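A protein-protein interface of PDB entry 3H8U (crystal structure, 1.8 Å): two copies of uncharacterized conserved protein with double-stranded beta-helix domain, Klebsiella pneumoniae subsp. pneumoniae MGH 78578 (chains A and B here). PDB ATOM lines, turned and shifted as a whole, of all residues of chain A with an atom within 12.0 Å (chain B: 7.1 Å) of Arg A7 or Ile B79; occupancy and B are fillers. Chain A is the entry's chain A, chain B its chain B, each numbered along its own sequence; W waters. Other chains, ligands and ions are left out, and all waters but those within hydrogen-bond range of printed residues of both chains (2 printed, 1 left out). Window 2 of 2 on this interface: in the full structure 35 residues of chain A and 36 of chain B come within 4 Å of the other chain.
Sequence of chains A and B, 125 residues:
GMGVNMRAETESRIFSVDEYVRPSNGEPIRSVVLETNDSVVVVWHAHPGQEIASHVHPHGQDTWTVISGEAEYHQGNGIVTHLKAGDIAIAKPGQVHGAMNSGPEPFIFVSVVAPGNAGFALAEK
The side-chain carboxylate (OE1) of Glu A11 lies close to the side-chain amide oxygen (OE1) of Gln B75 (3.0 Å).
The guanidinium group (NH2) of Arg A13 lies within hydrogen-bond range of the side-chain hydroxyl (OH) of Tyr B73 (3.0 Å).
NH1 of Arg A13 sits at hydrogen-bond distance from O of Gln B75 (3.4 Å).
O of Arg A7 sits at hydrogen-bond distance from OG of Ser A12 (2.7 Å).
The side-chain carboxylate (OE1) of Glu A11 is in salt-bridge range of the guanidinium group (NH1) of Arg A13.
The backbone NH of Tyr B73 lies within hydrogen-bond range of the backbone carbonyl oxygen of Thr B81, at 2.7 Å.
OG1 of Thr B81 sits at hydrogen-bond distance from NE2 of Gln B75 (2.9 Å).
Among the printed residues, pairs that only touch across the chains: Ile A14 with Thr B81 (3.2 Å) and Arg A7 with Ile B79 (3.7 Å).
Printed residues of chain B within 4 Å of Arg A7: Ile B79.
Ile B79 touches just one residue of chain A: Arg A7 (3.7 Å).
No residue of chain A comes within 4 Å of His B74.
Of chain A, only Glu A11 (3.0 Å) and Arg A13 (3.4 Å) come within 4 Å of Gln B75.
No residue of chain A comes within 4 Å of Asn B77.
Of the printed residues of chain B, Ile A14 touches Thr B81 (3.2 Å).
Of the printed residues of chain A, Tyr B73 touches Arg A13 (3.0 Å).
Of the printed residues of chain B, Arg A13 touches Tyr B73 and Gln B75.
Of the printed residues of chain A, Thr B81 touches Ile A14.
Printed residues of chain B within 4 Å of Glu A11: Gln B75 (3.0 Å).
Tyr A20 touches none of the printed residues of chain B.
Glu A9 touches none of the printed residues of chain B.
The nearest printed residue of chain B that does not touch Arg A7 is Thr B81 (4.01 Å).
Of the 14 printed residues of chain A, 4 touch a printed residue of chain B.
Hydrophobic or aromatic side chains of chain A within 4 Å of the printed part of chain B: Ile A14.
Along chain A the printed residues that touch a printed residue of chain B span positions 7 to 14.
Of the 11 printed residues of chain B, 4 touch a printed residue of chain A.
No position is printed for both chains.
Water W2 lies within hydrogen-bond range of NE2 of Gln B75 (2.7 Å), N of Arg A13 (3.1 Å) and O of Glu A11 (3.2 Å).
Water W1 lies within hydrogen-bond range of the backbone carbonyl oxygen (O) of Val B80, the guanidinium group (NH2) of Arg A7 and the side-chain amide nitrogen (ND2) of Asn A5.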
ATOM      1  N   VAL A   4       3.274   0.978 -22.111  1.00  0.00           N
ATOM      2  CA  VAL A   4       2.593  -0.054 -22.955  1.00  0.00           C
ATOM      3  C   VAL A   4       1.565  -0.809 -22.121  1.00  0.00           C
ATOM      4  O   VAL A   4       0.362  -0.596 -22.254  1.00  0.00           O
ATOM      5  N   ASN A   5       2.053  -1.692 -21.261  1.00  0.00           N
ATOM      6  CA  ASN A   5       1.193  -2.367 -20.296  1.00  0.00           C
ATOM      7  C   ASN A   5       0.982  -1.503 -19.061  1.00  0.00           C
ATOM      8  O   ASN A   5       1.873  -0.757 -18.639  1.00  0.00           O
ATOM      9  CB  ASN A   5       1.767  -3.729 -19.894  1.00  0.00           C
ATOM     10  CG  ASN A   5       1.636  -4.758 -20.991  1.00  0.00           C
ATOM     11  OD1 ASN A   5       1.137  -4.465 -22.084  1.00  0.00           O
ATOM     12  ND2 ASN A   5       2.066  -5.977 -20.707  1.00  0.00           N
ATOM     13  N   MET A   6      -0.220  -1.610 -18.499  1.00  0.00           N
ATOM     14  CA  MET A   6      -0.583  -0.893 -17.285  1.00  0.00           C
ATOM     15  C   MET A   6      -1.496  -1.765 -16.433  1.00  0.00           C
ATOM     16  O   MET A   6      -2.416  -2.388 -16.942  1.00  0.00           O
ATOM     17  CB  MET A   6      -1.298   0.404 -17.640  1.00  0.00           C
ATOM     18  CG  MET A   6      -1.297   1.421 -16.524  1.00  0.00           C
ATOM     19  SD  MET A   6      -0.786   3.168 -17.236  1.00  0.00           S
ATOM     20  CE  MET A   6       1.125   2.832 -17.558  1.00  0.00           C
ATOM     21  N   ARG A   7      -1.211  -1.814 -15.133  1.00  0.00           N
ATOM     22  CA  ARG A   7      -2.006  -2.606 -14.198  1.00  0.00           C
ATOM     23  C   ARG A   7      -2.512  -1.723 -13.054  1.00  0.00           C
ATOM     24  O   ARG A   7      -1.989  -0.624 -12.819  1.00  0.00           O
ATOM     25  CB  ARG A   7      -1.171  -3.772 -13.680  1.00  0.00           C
ATOM     26  CG  ARG A   7      -0.590  -4.626 -14.810  1.00  0.00           C
ATOM     27  CD  ARG A   7       0.223  -5.816 -14.298  1.00  0.00           C
ATOM     28  NE  ARG A   7       0.710  -6.652 -15.396  1.00  0.00           N
ATOM     29  CZ  ARG A   7       0.072  -7.682 -15.936  1.00  0.00           C
ATOM     30  NH1 ARG A   7      -1.139  -8.107 -15.508  1.00  0.00           N
ATOM     31  NH2 ARG A   7       0.669  -8.311 -16.939  1.00  0.00           N
ATOM     32  N   ALA A   8      -3.564  -2.189 -12.380  1.00  0.00           N
ATOM     33  CA  ALA A   8      -4.021  -1.584 -11.128  1.00  0.00           C
ATOM     34  C   ALA A   8      -2.839  -1.422 -10.157  1.00  0.00           C
ATOM     35  O   ALA A   8      -1.786  -2.084 -10.298  1.00  0.00           O
ATOM     36  CB  ALA A   8      -5.120  -2.437 -10.498  1.00  0.00           C
ATOM     37  N   GLU A   9      -3.017  -0.546  -9.170  1.00  0.00           N
ATOM     38  CA  GLU A   9      -1.899  -0.172  -8.291  1.00  0.00           C
ATOM     39  C   GLU A   9      -1.351  -1.386  -7.515  1.00  0.00           C
ATOM     40  O   GLU A   9      -0.138  -1.482  -7.318  1.00  0.00           O
ATOM     41  CB  GLU A   9      -2.283   0.992  -7.356  1.00  0.00           C
ATOM     42  CG  GLU A   9      -1.160   2.045  -7.188  1.00  0.00           C
ATOM     43  CD  GLU A   9      -1.691   3.478  -6.999  1.00  0.00           C
ATOM     44  OE1 GLU A   9      -2.932   3.667  -6.925  1.00  0.00           O
ATOM     45  OE2 GLU A   9      -0.862   4.415  -6.923  1.00  0.00           O
ATOM     46  N   THR A  10      -2.238  -2.316  -7.134  1.00  0.00           N
ATOM     47  CA  THR A  10      -1.842  -3.567  -6.456  1.00  0.00           C
ATOM     48  C   THR A  10      -0.767  -4.338  -7.223  1.00  0.00           C
ATOM     49  O   THR A  10       0.271  -4.686  -6.654  1.00  0.00           O
ATOM     50  CB  THR A  10      -3.021  -4.530  -6.279  1.00  0.00           C
ATOM     51  OG1 THR A  10      -3.630  -4.782  -7.557  1.00  0.00           O
ATOM     52  CG2 THR A  10      -4.068  -3.965  -5.295  1.00  0.00           C
ATOM     53  N   GLU A  11      -1.041  -4.584  -8.512  1.00  0.00           N
ATOM     54  CA  GLU A  11      -0.141  -5.330  -9.393  1.00  0.00           C
ATOM     55  C   GLU A  11       0.817  -4.451 -10.228  1.00  0.00           C
ATOM     56  O   GLU A  11       1.488  -4.991 -11.130  1.00  0.00           O
ATOM     57  CB  GLU A  11      -0.923  -6.289 -10.328  1.00  0.00           C
ATOM     58  CG  GLU A  11      -1.762  -7.388  -9.617  1.00  0.00           C
ATOM     59  CD  GLU A  11      -0.924  -8.505  -8.954  1.00  0.00           C
ATOM     60  OE1 GLU A  11       0.324  -8.507  -9.075  1.00  0.00           O
ATOM     61  OE2 GLU A  11      -1.527  -9.388  -8.295  1.00  0.00           O
ATOM     62  N   SER A  12       0.890  -3.149  -9.920  1.00  0.00           N
ATOM     63  CA  SER A  12       1.907  -2.244 -10.477  1.00  0.00           C
ATOM     64  C   SER A  12       3.195  -2.334  -9.638  1.00  0.00           C
ATOM     65  O   SER A  12       3.375  -1.619  -8.647  1.00  0.00           O
ATOM     66  CB  SER A  12       1.379  -0.813 -10.496  1.00  0.00           C
ATOM     67  OG  SER A  12       0.184  -0.732 -11.251  1.00  0.00           O
ATOM     68  N   ARG A  13       4.090  -3.227 -10.034  1.00  0.00           N
ATOM     69  CA  ARG A  13       5.091  -3.706  -9.109  1.00  0.00           C
ATOM     70  C   ARG A  13       6.506  -3.582  -9.567  1.00  0.00           C
ATOM     71  O   ARG A  13       7.388  -4.029  -8.825  1.00  0.00           O
ATOM     72  CB  ARG A  13       4.772  -5.171  -8.739  1.00  0.00           C
ATOM     73  CG  ARG A  13       3.505  -5.279  -7.860  1.00  0.00           C
ATOM     74  CD  ARG A  13       2.978  -6.660  -7.644  1.00  0.00           C
ATOM     75  NE  ARG A  13       4.033  -7.583  -7.230  1.00  0.00           N
ATOM     76  CZ  ARG A  13       3.842  -8.886  -7.044  1.00  0.00           C
ATOM     77  NH1 ARG A  13       2.654  -9.447  -7.236  1.00  0.00           N
ATOM     78  NH2 ARG A  13       4.872  -9.636  -6.672  1.00  0.00           N
ATOM     79  N   ILE A  14       6.726  -3.025 -10.758  1.00  0.00           N
ATOM     80  CA  ILE A  14       8.067  -2.872 -11.314  1.00  0.00           C
ATOM     81  C   ILE A  14       8.229  -1.369 -11.513  1.00  0.00           C
ATOM     82  O   ILE A  14       7.339  -0.699 -12.088  1.00  0.00           O
ATOM     83  CB  ILE A  14       8.252  -3.646 -12.622  1.00  0.00           C
ATOM     84  CG1 ILE A  14       8.059  -5.137 -12.393  1.00  0.00           C
ATOM     85  CG2 ILE A  14       9.622  -3.387 -13.268  1.00  0.00           C
ATOM     86  CD1 ILE A  14       8.255  -5.942 -13.586  1.00  0.00           C
ATOM     87  N   PHE A  15       9.363  -0.859 -11.047  1.00  0.00           N
ATOM     88  CA  PHE A  15       9.689   0.542 -11.091  1.00  0.00           C
ATOM     89  C   PHE A  15      11.107   0.668 -11.652  1.00  0.00           C
ATOM     90  O   PHE A  15      12.062   0.076 -11.138  1.00  0.00           O
ATOM     91  CB  PHE A  15       9.642   1.159  -9.692  1.00  0.00           C
ATOM     92  CG  PHE A  15       8.353   0.940  -8.974  1.00  0.00           C
ATOM     93  CD1 PHE A  15       8.102  -0.248  -8.316  1.00  0.00           C
ATOM     94  CD2 PHE A  15       7.377   1.919  -8.946  1.00  0.00           C
ATOM     95  CE1 PHE A  15       6.865  -0.472  -7.626  1.00  0.00           C
ATOM     96  CE2 PHE A  15       6.129   1.699  -8.260  1.00  0.00           C
ATOM     97  CZ  PHE A  15       5.894   0.508  -7.614  1.00  0.00           C
ATOM     98  N   TYR A  20      12.807   7.451 -11.856  1.00  0.00           N
ATOM     99  CA  TYR A  20      12.738   8.088 -10.531  1.00  0.00           C
ATOM    100  C   TYR A  20      13.992   8.903 -10.173  1.00  0.00           C
ATOM    101  O   TYR A  20      14.029   9.601  -9.161  1.00  0.00           O
ATOM    102  CB  TYR A  20      12.480   7.012  -9.471  1.00  0.00           C
ATOM    103  CG  TYR A  20      11.043   6.536  -9.494  1.00  0.00           C
ATOM    104  CD1 TYR A  20      10.626   5.581 -10.435  1.00  0.00           C
ATOM    105  CD2 TYR A  20      10.100   7.064  -8.639  1.00  0.00           C
ATOM    106  CE1 TYR A  20       9.314   5.176 -10.513  1.00  0.00           C
ATOM    107  CE2 TYR A  20       8.768   6.649  -8.711  1.00  0.00           C
ATOM    108  CZ  TYR A  20       8.402   5.705  -9.651  1.00  0.00           C
ATOM    109  OH  TYR A  20       7.124   5.256  -9.708  1.00  0.00           O
ATOM    110  N   LEU A  34       8.147   4.083  -3.439  1.00  0.00           N
ATOM    111  CA  LEU A  34       6.974   3.553  -2.760  1.00  0.00           C
ATOM    112  C   LEU A  34       7.171   3.574  -1.250  1.00  0.00           C
ATOM    113  O   LEU A  34       8.215   3.132  -0.744  1.00  0.00           O
ATOM    114  CB  LEU A  34       6.720   2.118  -3.223  1.00  0.00           C
ATOM    115  CG  LEU A  34       5.338   1.540  -2.839  1.00  0.00           C
ATOM    116  CD1 LEU A  34       4.284   2.146  -3.733  1.00  0.00           C
ATOM    117  CD2 LEU A  34       5.294   0.017  -2.866  1.00  0.00           C
ATOM    118  N   GLU B  72      12.123 -12.708 -16.412  1.00  0.00           N
ATOM    119  CA  GLU B  72      10.685 -12.616 -16.227  1.00  0.00           C
ATOM    120  C   GLU B  72      10.355 -12.623 -14.726  1.00  0.00           C
ATOM    121  O   GLU B  72      10.785 -13.500 -13.996  1.00  0.00           O
ATOM    122  CB  GLU B  72      10.029 -13.765 -16.988  1.00  0.00           C
ATOM    123  CG  GLU B  72      10.162 -13.558 -18.508  1.00  0.00           C
ATOM    124  CD  GLU B  72      10.000 -14.814 -19.361  1.00  0.00           C
ATOM    125  OE1 GLU B  72       9.580 -15.887 -18.841  1.00  0.00           O
ATOM    126  OE2 GLU B  72      10.300 -14.702 -20.592  1.00  0.00           O
ATOM    127  N   TYR B  73       9.654 -11.602 -14.261  1.00  0.00           N
ATOM    128  CA  TYR B  73       9.162 -11.531 -12.886  1.00  0.00           C
ATOM    129  C   TYR B  73       7.785 -12.189 -12.841  1.00  0.00           C
ATOM    130  O   TYR B  73       6.893 -11.851 -13.629  1.00  0.00           O
ATOM    131  CB  TYR B  73       9.044 -10.070 -12.487  1.00  0.00           C
ATOM    132  CG  TYR B  73       8.693  -9.776 -11.041  1.00  0.00           C
ATOM    133  CD1 TYR B  73       9.440 -10.298  -9.982  1.00  0.00           C
ATOM    134  CD2 TYR B  73       7.643  -8.917 -10.739  1.00  0.00           C
ATOM    135  CE1 TYR B  73       9.131  -9.980  -8.650  1.00  0.00           C
ATOM    136  CE2 TYR B  73       7.314  -8.606  -9.420  1.00  0.00           C
ATOM    137  CZ  TYR B  73       8.070  -9.137  -8.376  1.00  0.00           C
ATOM    138  OH  TYR B  73       7.750  -8.841  -7.072  1.00  0.00           O
ATOM    139  N   HIS B  74       7.632 -13.152 -11.947  1.00  0.00           N
ATOM    140  CA  HIS B  74       6.396 -13.894 -11.756  1.00  0.00           C
ATOM    141  C   HIS B  74       5.624 -13.248 -10.609  1.00  0.00           C
ATOM    142  O   HIS B  74       6.122 -13.156  -9.481  1.00  0.00           O
ATOM    143  CB  HIS B  74       6.714 -15.347 -11.438  1.00  0.00           C
ATOM    144  CG  HIS B  74       7.416 -16.049 -12.551  1.00  0.00           C
ATOM    145  ND1 HIS B  74       8.175 -17.183 -12.354  1.00  0.00           N
ATOM    146  CD2 HIS B  74       7.479 -15.771 -13.875  1.00  0.00           C
ATOM    147  CE1 HIS B  74       8.635 -17.598 -13.523  1.00  0.00           C
ATOM    148  NE2 HIS B  74       8.238 -16.754 -14.463  1.00  0.00           N
ATOM    149  N   GLN B  75       4.431 -12.765 -10.923  1.00  0.00           N
ATOM    150  CA  GLN B  75       3.610 -12.054  -9.957  1.00  0.00           C
ATOM    151  C   GLN B  75       2.463 -12.889  -9.396  1.00  0.00           C
ATOM    152  O   GLN B  75       1.637 -12.369  -8.662  1.00  0.00           O
ATOM    153  CB  GLN B  75       3.089 -10.738 -10.553  1.00  0.00           C
ATOM    154  CG  GLN B  75       4.173  -9.768 -10.998  1.00  0.00           C
ATOM    155  CD  GLN B  75       3.641  -8.388 -11.396  1.00  0.00           C
ATOM    156  OE1 GLN B  75       2.499  -8.011 -11.106  1.00  0.00           O
ATOM    157  NE2 GLN B  75       4.469  -7.637 -12.045  1.00  0.00           N
ATOM    158  N   GLY B  76       2.419 -14.185  -9.728  1.00  0.00           N
ATOM    159  CA  GLY B  76       1.349 -15.051  -9.343  1.00  0.00           C
ATOM    160  C   GLY B  76       0.246 -14.991 -10.387  1.00  0.00           C
ATOM    161  O   GLY B  76       0.227 -14.058 -11.196  1.00  0.00           O
ATOM    162  N   ASN B  77      -0.671 -15.954 -10.348  1.00  0.00           N
ATOM    163  CA  ASN B  77      -1.825 -15.967 -11.258  1.00  0.00           C
ATOM    164  C   ASN B  77      -1.437 -15.888 -12.751  1.00  0.00           C
ATOM    165  O   ASN B  77      -2.166 -15.336 -13.579  1.00  0.00           O
ATOM    166  CB  ASN B  77      -2.750 -14.801 -10.872  1.00  0.00           C
ATOM    167  CG  ASN B  77      -3.337 -14.965  -9.475  1.00  0.00           C
ATOM    168  OD1 ASN B  77      -2.995 -14.229  -8.539  1.00  0.00           O
ATOM    169  ND2 ASN B  77      -4.158 -15.951  -9.316  1.00  0.00           N
ATOM    170  N   GLY B  78      -0.272 -16.437 -13.071  1.00  0.00           N
ATOM    171  CA  GLY B  78       0.220 -16.481 -14.444  1.00  0.00           C
ATOM    172  C   GLY B  78       0.719 -15.147 -14.963  1.00  0.00           C
ATOM    173  O   GLY B  78       0.989 -15.010 -16.160  1.00  0.00           O
ATOM    174  N   ILE B  79       0.812 -14.152 -14.096  1.00  0.00           N
ATOM    175  CA  ILE B  79       1.227 -12.828 -14.507  1.00  0.00           C
ATOM    176  C   ILE B  79       2.730 -12.823 -14.642  1.00  0.00           C
ATOM    177  O   ILE B  79       3.468 -13.177 -13.690  1.00  0.00           O
ATOM    178  CB  ILE B  79       0.801 -11.744 -13.495  1.00  0.00           C
ATOM    179  CG1 ILE B  79      -0.727 -11.678 -13.391  1.00  0.00           C
ATOM    180  CG2 ILE B  79       1.453 -10.397 -13.842  1.00  0.00           C
ATOM    181  CD1 ILE B  79      -1.185 -10.876 -12.228  1.00  0.00           C
ATOM    182  N   VAL B  80       3.189 -12.392 -15.811  1.00  0.00           N
ATOM    183  CA  VAL B  80       4.617 -12.343 -16.104  1.00  0.00           C
ATOM    184  C   VAL B  80       4.956 -10.950 -16.633  1.00  0.00           C
ATOM    185  O   VAL B  80       4.405 -10.493 -17.628  1.00  0.00           O
ATOM    186  CB  VAL B  80       5.027 -13.384 -17.154  1.00  0.00           C
ATOM    187  CG1 VAL B  80       6.552 -13.242 -17.457  1.00  0.00           C
ATOM    188  CG2 VAL B  80       4.668 -14.793 -16.706  1.00  0.00           C
ATOM    189  N   THR B  81       5.896 -10.290 -15.976  1.00  0.00           N
ATOM    190  CA  THR B  81       6.362  -8.966 -16.397  1.00  0.00           C
ATOM    191  C   THR B  81       7.861  -9.084 -16.556  1.00  0.00           C
ATOM    192  O   THR B  81       8.478  -9.978 -16.023  1.00  0.00           O
ATOM    193  CB  THR B  81       6.013  -7.931 -15.335  1.00  0.00           C
ATOM    194  OG1 THR B  81       6.381  -8.451 -14.037  1.00  0.00           O
ATOM    195  CG2 THR B  81       4.578  -7.696 -15.296  1.00  0.00           C
ATOM    196  N   LYS B 125       3.558 -19.712  -9.641  1.00  0.00           N
ATOM    197  CA  LYS B 125       3.639 -18.655 -10.603  1.00  0.00           C
ATOM    198  C   LYS B 125       2.312 -18.540 -11.353  1.00  0.00           C
ATOM    199  O   LYS B 125       1.989 -17.423 -11.757  1.00  0.00           O
ATOM    200  CB  LYS B 125       4.794 -18.856 -11.555  1.00  0.00           C
ATOM    201  CG  LYS B 125       4.658 -19.979 -12.509  1.00  0.00           C
ATOM    202  CD  LYS B 125       5.657 -19.783 -13.646  1.00  0.00           C
ATOM    203  CE  LYS B 125       5.683 -21.008 -14.553  1.00  0.00           C
ATOM    204  NZ  LYS B 125       6.801 -20.954 -15.540  1.00  0.00           N
ATOM    205  OXT LYS B 125       1.574 -19.533 -11.527  1.00  0.00           O
HETATM  206  O   HOH W   1       3.204  -8.239 -18.531  1.00  0.00           O
HETATM  207  O   HOH W   2       4.338  -4.988 -12.523  1.00  0.00           O
